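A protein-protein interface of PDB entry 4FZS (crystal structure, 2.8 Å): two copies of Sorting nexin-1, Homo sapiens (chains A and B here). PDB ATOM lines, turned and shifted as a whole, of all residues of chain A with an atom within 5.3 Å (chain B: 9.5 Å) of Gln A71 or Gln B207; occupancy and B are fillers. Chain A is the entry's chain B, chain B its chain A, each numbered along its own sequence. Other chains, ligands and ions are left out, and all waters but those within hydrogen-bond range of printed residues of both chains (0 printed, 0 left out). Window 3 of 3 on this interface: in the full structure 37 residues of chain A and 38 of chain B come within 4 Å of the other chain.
The backbone carbonyl oxygen (O) of Arg A67 sits close to the side-chain amide nitrogen (NE2) of Gln A71 (3.5 Å).
Among the printed residues, merely in contact across the chains: Ala A68 with Leu B199 (3.8 Å), Leu A69 with Leu B199 (3.8 Å), Gln A71 with Leu B203 (3.5 Å), Gln A71 with Gln B207 (3.9 Å), Leu A72 with Leu B199 (3.9 Å), Leu A72 with Leu B202 (3.8 Å), Leu A72 with Leu B203 (3.6 Å), Val A75 with Leu B203 (3.7 Å) and Val A75 with Gln B206 (3.7 Å).
Gln A71 touches just these residues of chain B: Leu B203 and Gln B207. No residue of chain B comes within 4 Å of Ser A70. No residue of chain B comes within 4 Å of Glu A74. Printed residues of chain B within 4 Å of Ala A68: Leu B199. Printed residues of chain B within 4 Å of Leu A72: Leu B199 (3.9 Å), Leu B202 (3.8 Å) and Leu B203 (3.6 Å). Of the printed residues of chain A, Leu B202 touches Leu A72 (3.8 Å). Of the printed residues of chain A, Leu B203 touches Gln A71, Leu A72 and Val A75. Glu B200 touches none of the printed residues of chain A. Ala B210 touches none of the printed residues of chain A. The nearest residue of chain B that does not touch Gln A71 is Glu B200 (7.2 Å). The nearest residue of chain A that does not touch Gln B207 is Val A75 (4.3 Å).
Printed residues of chain B that touch a printed residue of chain A: Leu B199, Leu B202, Leu B203, Gln B206 and Gln B207. Hydrophobic or aromatic side chains of chain B within 4 Å of the printed part of chain A: Leu B199, Leu B202 and Leu B203. Of the 10 printed residues of chain A, 5 touch a printed residue of chain B. Printed residues of chain A that touch a printed residue of chain B: Ala A68, Leu A69, Gln A71, Leu A72 and Val A75. Hydrophobic or aromatic side chains of chain A within 4 Å of the printed part of chain B: Ala A68, Leu A69, Leu A72 and Val A75. Among the printed residues, 9 pairs touch across the chains. Among the printed residues, no Asp or Glu carboxylate lies within 4 Å of a Lys or Arg side-chain nitrogen of the other chain.
No position is printed for both chains. Of the 9 pairs that touch across the chains among the printed residues, none has its exchanged pair printed and touching as well.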
ATOM      1  N   SER A  66      14.307  22.219  14.662  1.00  0.00           N
ATOM      2  CA  SER A  66      13.521  21.591  15.724  1.00  0.00           C
ATOM      3  C   SER A  66      12.060  22.015  15.672  1.00  0.00           C
ATOM      4  O   SER A  66      11.195  21.131  15.656  1.00  0.00           O
ATOM      5  CB  SER A  66      14.110  21.866  17.104  1.00  0.00           C
ATOM      6  OG  SER A  66      13.314  21.236  18.099  1.00  0.00           O
ATOM      7  N   ARG A  67      11.792  23.356  15.605  1.00  0.00           N
ATOM      8  CA  ARG A  67      10.437  23.919  15.540  1.00  0.00           C
ATOM      9  C   ARG A  67       9.711  23.455  14.291  1.00  0.00           C
ATOM     10  O   ARG A  67       8.562  23.033  14.395  1.00  0.00           O
ATOM     11  CB  ARG A  67      10.453  25.461  15.592  1.00  0.00           C
ATOM     12  CG  ARG A  67      10.134  26.039  16.964  1.00  0.00           C
ATOM     13  CD  ARG A  67      10.408  27.547  17.084  1.00  0.00           C
ATOM     14  NE  ARG A  67      11.356  27.867  18.171  1.00  0.00           N
ATOM     15  CZ  ARG A  67      11.366  28.996  18.885  1.00  0.00           C
ATOM     16  NH1 ARG A  67      10.477  29.957  18.642  1.00  0.00           N
ATOM     17  NH2 ARG A  67      12.258  29.168  19.852  1.00  0.00           N
ATOM     18  N   ALA A  68      10.384  23.501  13.119  1.00  0.00           N
ATOM     19  CA  ALA A  68       9.779  23.099  11.860  1.00  0.00           C
ATOM     20  C   ALA A  68       9.322  21.657  11.906  1.00  0.00           C
ATOM     21  O   ALA A  68       8.170  21.392  11.533  1.00  0.00           O
ATOM     22  CB  ALA A  68      10.727  23.327  10.686  1.00  0.00           C
ATOM     23  N   LEU A  69      10.177  20.736  12.432  1.00  0.00           N
ATOM     24  CA  LEU A  69       9.830  19.316  12.534  1.00  0.00           C
ATOM     25  C   LEU A  69       8.661  19.113  13.479  1.00  0.00           C
ATOM     26  O   LEU A  69       7.721  18.403  13.121  1.00  0.00           O
ATOM     27  CB  LEU A  69      11.014  18.445  12.948  1.00  0.00           C
ATOM     28  CG  LEU A  69      12.193  18.328  11.990  1.00  0.00           C
ATOM     29  CD1 LEU A  69      13.483  18.023  12.754  1.00  0.00           C
ATOM     30  CD2 LEU A  69      11.943  17.274  10.955  1.00  0.00           C
ATOM     31  N   SER A  70       8.672  19.757  14.646  1.00  0.00           N
ATOM     32  CA  SER A  70       7.547  19.579  15.563  1.00  0.00           C
ATOM     33  C   SER A  70       6.230  20.226  15.113  1.00  0.00           C
ATOM     34  O   SER A  70       5.169  19.644  15.322  1.00  0.00           O
ATOM     35  CB  SER A  70       7.930  19.869  17.014  1.00  0.00           C
ATOM     36  OG  SER A  70       8.764  21.001  17.169  1.00  0.00           O
ATOM     37  N   GLN A  71       6.304  21.357  14.409  1.00  0.00           N
ATOM     38  CA  GLN A  71       5.113  22.004  13.867  1.00  0.00           C
ATOM     39  C   GLN A  71       4.470  21.151  12.741  1.00  0.00           C
ATOM     40  O   GLN A  71       3.256  21.070  12.681  1.00  0.00           O
ATOM     41  CB  GLN A  71       5.460  23.390  13.346  1.00  0.00           C
ATOM     42  CG  GLN A  71       5.628  24.424  14.434  1.00  0.00           C
ATOM     43  CD  GLN A  71       5.952  25.749  13.835  1.00  0.00           C
ATOM     44  OE1 GLN A  71       5.106  26.371  13.199  1.00  0.00           O
ATOM     45  NE2 GLN A  71       7.179  26.222  14.027  1.00  0.00           N
ATOM     46  N   LEU A  72       5.291  20.499  11.885  1.00  0.00           N
ATOM     47  CA  LEU A  72       4.860  19.610  10.803  1.00  0.00           C
ATOM     48  C   LEU A  72       4.230  18.359  11.388  1.00  0.00           C
ATOM     49  O   LEU A  72       3.337  17.781  10.765  1.00  0.00           O
ATOM     50  CB  LEU A  72       6.056  19.187   9.939  1.00  0.00           C
ATOM     51  CG  LEU A  72       5.976  19.246   8.376  1.00  0.00           C
ATOM     52  CD1 LEU A  72       6.798  18.143   7.765  1.00  0.00           C
ATOM     53  CD2 LEU A  72       4.568  19.100   7.841  1.00  0.00           C
ATOM     54  N   ALA A  73       4.712  17.912  12.571  1.00  0.00           N
ATOM     55  CA  ALA A  73       4.154  16.744  13.259  1.00  0.00           C
ATOM     56  C   ALA A  73       2.738  17.120  13.688  1.00  0.00           C
ATOM     57  O   ALA A  73       1.811  16.400  13.334  1.00  0.00           O
ATOM     58  CB  ALA A  73       5.024  16.358  14.462  1.00  0.00           C
ATOM     59  N   GLU A  74       2.565  18.319  14.327  1.00  0.00           N
ATOM     60  CA  GLU A  74       1.267  18.866  14.758  1.00  0.00           C
ATOM     61  C   GLU A  74       0.296  18.996  13.564  1.00  0.00           C
ATOM     62  O   GLU A  74      -0.895  18.738  13.719  1.00  0.00           O
ATOM     63  CB  GLU A  74       1.431  20.238  15.430  1.00  0.00           C
ATOM     64  CG  GLU A  74       1.967  20.193  16.848  1.00  0.00           C
ATOM     65  CD  GLU A  74       2.146  21.536  17.542  1.00  0.00           C
ATOM     66  OE1 GLU A  74       1.162  22.312  17.596  1.00  0.00           O
ATOM     67  OE2 GLU A  74       3.256  21.790  18.070  1.00  0.00           O
ATOM     68  N   VAL A  75       0.806  19.369  12.377  1.00  0.00           N
ATOM     69  CA  VAL A  75      -0.008  19.539  11.182  1.00  0.00           C
ATOM     70  C   VAL A  75      -0.503  18.216  10.620  1.00  0.00           C
ATOM     71  O   VAL A  75      -1.711  18.111  10.403  1.00  0.00           O
ATOM     72  CB  VAL A  75       0.611  20.488  10.116  1.00  0.00           C
ATOM     73  CG1 VAL A  75      -0.285  20.618   8.900  1.00  0.00           C
ATOM     74  CG2 VAL A  75       0.836  21.868  10.702  1.00  0.00           C
ATOM     75  N   LEU B 199      11.521  22.539   4.513  1.00  0.00           N
ATOM     76  CA  LEU B 199      10.626  22.199   5.604  1.00  0.00           C
ATOM     77  C   LEU B 199       9.606  23.290   5.933  1.00  0.00           C
ATOM     78  O   LEU B 199       8.442  22.982   6.148  1.00  0.00           O
ATOM     79  CB  LEU B 199      11.430  21.893   6.851  1.00  0.00           C
ATOM     80  CG  LEU B 199      11.651  20.440   7.233  1.00  0.00           C
ATOM     81  CD1 LEU B 199      12.053  20.381   8.696  1.00  0.00           C
ATOM     82  CD2 LEU B 199      10.391  19.599   7.043  1.00  0.00           C
ATOM     83  N   GLU B 200      10.043  24.559   5.955  1.00  0.00           N
ATOM     84  CA  GLU B 200       9.199  25.721   6.242  1.00  0.00           C
ATOM     85  C   GLU B 200       8.171  25.957   5.157  1.00  0.00           C
ATOM     86  O   GLU B 200       7.034  26.284   5.484  1.00  0.00           O
ATOM     87  CB  GLU B 200      10.042  26.955   6.493  1.00  0.00           C
ATOM     88  CG  GLU B 200      10.811  26.881   7.803  1.00  0.00           C
ATOM     89  CD  GLU B 200      11.787  28.008   8.076  1.00  0.00           C
ATOM     90  OE1 GLU B 200      12.046  28.815   7.154  1.00  0.00           O
ATOM     91  OE2 GLU B 200      12.307  28.074   9.214  1.00  0.00           O
ATOM     92  N   THR B 201       8.545  25.768   3.872  1.00  0.00           N
ATOM     93  CA  THR B 201       7.605  25.910   2.750  1.00  0.00           C
ATOM     94  C   THR B 201       6.597  24.765   2.770  1.00  0.00           C
ATOM     95  O   THR B 201       5.413  25.005   2.563  1.00  0.00           O
ATOM     96  CB  THR B 201       8.274  26.187   1.376  1.00  0.00           C
ATOM     97  OG1 THR B 201       8.077  25.075   0.497  1.00  0.00           O
ATOM     98  CG2 THR B 201       9.744  26.539   1.473  1.00  0.00           C
ATOM     99  N   LEU B 202       7.053  23.543   3.048  1.00  0.00           N
ATOM    100  CA  LEU B 202       6.193  22.364   3.186  1.00  0.00           C
ATOM    101  C   LEU B 202       5.155  22.641   4.290  1.00  0.00           C
ATOM    102  O   LEU B 202       3.965  22.502   4.044  1.00  0.00           O
ATOM    103  CB  LEU B 202       7.059  21.161   3.608  1.00  0.00           C
ATOM    104  CG  LEU B 202       6.731  19.764   3.092  1.00  0.00           C
ATOM    105  CD1 LEU B 202       7.138  18.767   4.079  1.00  0.00           C
ATOM    106  CD2 LEU B 202       5.243  19.566   2.718  1.00  0.00           C
ATOM    107  N   LEU B 203       5.627  23.087   5.483  1.00  0.00           N
ATOM    108  CA  LEU B 203       4.825  23.464   6.651  1.00  0.00           C
ATOM    109  C   LEU B 203       3.786  24.518   6.280  1.00  0.00           C
ATOM    110  O   LEU B 203       2.600  24.294   6.519  1.00  0.00           O
ATOM    111  CB  LEU B 203       5.742  24.011   7.756  1.00  0.00           C
ATOM    112  CG  LEU B 203       5.373  23.787   9.233  1.00  0.00           C
ATOM    113  CD1 LEU B 203       5.293  25.063   9.987  1.00  0.00           C
ATOM    114  CD2 LEU B 203       4.144  22.917   9.429  1.00  0.00           C
ATOM    115  N   TYR B 204       4.223  25.644   5.654  1.00  0.00           N
ATOM    116  CA  TYR B 204       3.348  26.748   5.246  1.00  0.00           C
ATOM    117  C   TYR B 204       2.259  26.247   4.329  1.00  0.00           C
ATOM    118  O   TYR B 204       1.086  26.496   4.580  1.00  0.00           O
ATOM    119  CB  TYR B 204       4.156  27.887   4.608  1.00  0.00           C
ATOM    120  CG  TYR B 204       3.310  28.986   4.021  1.00  0.00           C
ATOM    121  CD1 TYR B 204       2.732  29.953   4.835  1.00  0.00           C
ATOM    122  CD2 TYR B 204       3.083  29.058   2.647  1.00  0.00           C
ATOM    123  CE1 TYR B 204       1.925  30.955   4.300  1.00  0.00           C
ATOM    124  CE2 TYR B 204       2.275  30.048   2.099  1.00  0.00           C
ATOM    125  CZ  TYR B 204       1.707  31.004   2.926  1.00  0.00           C
ATOM    126  OH  TYR B 204       0.920  31.979   2.354  1.00  0.00           O
ATOM    127  N   SER B 205       2.652  25.514   3.287  1.00  0.00           N
ATOM    128  CA  SER B 205       1.782  24.905   2.292  1.00  0.00           C
ATOM    129  C   SER B 205       0.696  24.069   2.964  1.00  0.00           C
ATOM    130  O   SER B 205      -0.472  24.261   2.646  1.00  0.00           O
ATOM    131  CB  SER B 205       2.621  24.084   1.316  1.00  0.00           C
ATOM    132  OG  SER B 205       1.936  22.993   0.736  1.00  0.00           O
ATOM    133  N   GLN B 206       1.076  23.197   3.921  1.00  0.00           N
ATOM    134  CA  GLN B 206       0.180  22.321   4.690  1.00  0.00           C
ATOM    135  C   GLN B 206      -0.768  23.109   5.595  1.00  0.00           C
ATOM    136  O   GLN B 206      -1.944  22.764   5.694  1.00  0.00           O
ATOM    137  CB  GLN B 206       0.989  21.293   5.504  1.00  0.00           C
ATOM    138  CG  GLN B 206       1.653  20.165   4.702  1.00  0.00           C
ATOM    139  CD  GLN B 206       0.686  19.450   3.787  1.00  0.00           C
ATOM    140  OE1 GLN B 206       0.725  19.615   2.571  1.00  0.00           O
ATOM    141  NE2 GLN B 206      -0.169  18.610   4.334  1.00  0.00           N
ATOM    142  N   GLN B 207      -0.258  24.186   6.227  1.00  0.00           N
ATOM    143  CA  GLN B 207      -1.029  25.099   7.086  1.00  0.00           C
ATOM    144  C   GLN B 207      -2.132  25.761   6.258  1.00  0.00           C
ATOM    145  O   GLN B 207      -3.277  25.810   6.717  1.00  0.00           O
ATOM    146  CB  GLN B 207      -0.116  26.193   7.710  1.00  0.00           C
ATOM    147  CG  GLN B 207       0.896  25.687   8.753  1.00  0.00           C
ATOM    148  CD  GLN B 207       1.856  26.741   9.289  1.00  0.00           C
ATOM    149  OE1 GLN B 207       2.354  27.630   8.574  1.00  0.00           O
ATOM    150  NE2 GLN B 207       2.192  26.616  10.564  1.00  0.00           N
ATOM    151  N   GLN B 208      -1.790  26.242   5.027  1.00  0.00           N
ATOM    152  CA  GLN B 208      -2.756  26.902   4.132  1.00  0.00           C
ATOM    153  C   GLN B 208      -3.844  25.947   3.662  1.00  0.00           C
ATOM    154  O   GLN B 208      -4.968  26.394   3.492  1.00  0.00           O
ATOM    155  CB  GLN B 208      -2.104  27.625   2.951  1.00  0.00           C
ATOM    156  CG  GLN B 208      -1.127  28.737   3.327  1.00  0.00           C
ATOM    157  CD  GLN B 208      -1.716  29.879   4.137  1.00  0.00           C
ATOM    158  OE1 GLN B 208      -2.528  30.678   3.642  1.00  0.00           O
ATOM    159  NE2 GLN B 208      -1.259  30.018   5.385  1.00  0.00           N
ATOM    160  N   LEU B 209      -3.529  24.642   3.499  1.00  0.00           N
ATOM    161  CA  LEU B 209      -4.492  23.627   3.107  1.00  0.00           C
ATOM    162  C   LEU B 209      -5.495  23.433   4.251  1.00  0.00           C
ATOM    163  O   LEU B 209      -6.704  23.367   3.990  1.00  0.00           O
ATOM    164  CB  LEU B 209      -3.771  22.297   2.813  1.00  0.00           C
ATOM    165  CG  LEU B 209      -4.441  21.235   1.926  1.00  0.00           C
ATOM    166  CD1 LEU B 209      -3.904  19.832   2.236  1.00  0.00           C
ATOM    167  CD2 LEU B 209      -5.942  21.272   1.917  1.00  0.00           C
ATOM    168  N   ALA B 210      -4.990  23.351   5.506  1.00  0.00           N
ATOM    169  CA  ALA B 210      -5.810  23.167   6.703  1.00  0.00           C
ATOM    170  C   ALA B 210      -6.808  24.351   6.879  1.00  0.00           C
ATOM    171  O   ALA B 210      -8.003  24.126   7.092  1.00  0.00           O
ATOM    172  CB  ALA B 210      -4.916  22.990   7.926  1.00  0.00           C
ATOM    173  N   LYS B 211      -6.323  25.586   6.683  1.00  0.00           N
ATOM    174  CA  LYS B 211      -7.115  26.821   6.738  1.00  0.00           C
ATOM    175  C   LYS B 211      -8.183  26.874   5.618  1.00  0.00           C
ATOM    176  O   LYS B 211      -9.323  27.248   5.886  1.00  0.00           O
ATOM    177  CB  LYS B 211      -6.192  28.059   6.652  1.00  0.00           C
ATOM    178  CG  LYS B 211      -5.413  28.387   7.929  1.00  0.00           C
ATOM    179  CD  LYS B 211      -4.190  29.246   7.623  1.00  0.00           C
ATOM    180  CE  LYS B 211      -3.280  29.418   8.815  1.00  0.00           C
ATOM    181  NZ  LYS B 211      -1.929  29.917   8.421  1.00  0.00           N
ATOM    182  N   TYR B 212      -7.808  26.504   4.376  1.00  0.00           N
ATOM    183  CA  TYR B 212      -8.696  26.495   3.207  1.00  0.00           C
ATOM    184  C   TYR B 212      -9.802  25.480   3.354  1.00  0.00           C
ATOM    185  O   TYR B 212     -10.944  25.821   3.077  1.00  0.00           O
ATOM    186  CB  TYR B 212      -7.907  26.235   1.923  1.00  0.00           C
ATOM    187  CG  TYR B 212      -8.742  26.065   0.676  1.00  0.00           C
ATOM    188  CD1 TYR B 212      -9.266  24.821   0.328  1.00  0.00           C
ATOM    189  CD2 TYR B 212      -8.931  27.122  -0.208  1.00  0.00           C
ATOM    190  CE1 TYR B 212      -9.994  24.646  -0.841  1.00  0.00           C
ATOM    191  CE2 TYR B 212      -9.646  26.956  -1.387  1.00  0.00           C
ATOM    192  CZ  TYR B 212     -10.168  25.714  -1.705  1.00  0.00           C
ATOM    193  OH  TYR B 212     -10.824  25.533  -2.899  1.00  0.00           O
ATOM    194  N   TRP B 213      -9.475  24.240   3.763  1.00  0.00           N
ATOM    195  CA  TRP B 213     -10.442  23.158   3.952  1.00  0.00           C
ATOM    196  C   TRP B 213     -11.570  23.469   4.951  1.00  0.00           C
ATOM    197  O   TRP B 213     -12.641  22.870   4.852  1.00  0.00           O
ATOM    198  CB  TRP B 213      -9.742  21.828   4.271  1.00  0.00           C
ATOM    199  CG  TRP B 213     -10.327  20.688   3.503  1.00  0.00           C
ATOM    200  CD1 TRP B 213     -11.151  19.717   3.988  1.00  0.00           C
ATOM    201  CD2 TRP B 213     -10.262  20.488   2.077  1.00  0.00           C
ATOM    202  NE1 TRP B 213     -11.562  18.890   2.964  1.00  0.00           N
ATOM    203  CE2 TRP B 213     -11.042  19.352   1.778  1.00  0.00           C
ATOM    204  CE3 TRP B 213      -9.591  21.147   1.025  1.00  0.00           C
ATOM    205  CZ2 TRP B 213     -11.161  18.847   0.472  1.00  0.00           C
ATOM    206  CZ3 TRP B 213      -9.709  20.646  -0.266  1.00  0.00           C
ATOM    207  CH2 TRP B 213     -10.477  19.506  -0.530  1.00  0.00           C
ATOM    208  N   GLU B 214     -11.352  24.448   5.863  1.00  0.00           N
ATOM    209  CA  GLU B 214     -12.343  24.894   6.850  1.00  0.00           C
ATOM    210  C   GLU B 214     -13.592  25.575   6.215  1.00  0.00           C
ATOM    211  O   GLU B 214     -14.566  25.833   6.931  1.00  0.00           O
ATOM    212  CB  GLU B 214     -11.687  25.780   7.928  1.00  0.00           C
ATOM    213  CG  GLU B 214     -10.901  24.997   8.976  1.00  0.00           C
ATOM    214  CD  GLU B 214      -9.880  25.772   9.795  1.00  0.00           C
ATOM    215  OE1 GLU B 214      -9.935  27.025   9.815  1.00  0.00           O
ATOM    216  OE2 GLU B 214      -9.018  25.117  10.427  1.00  0.00           O
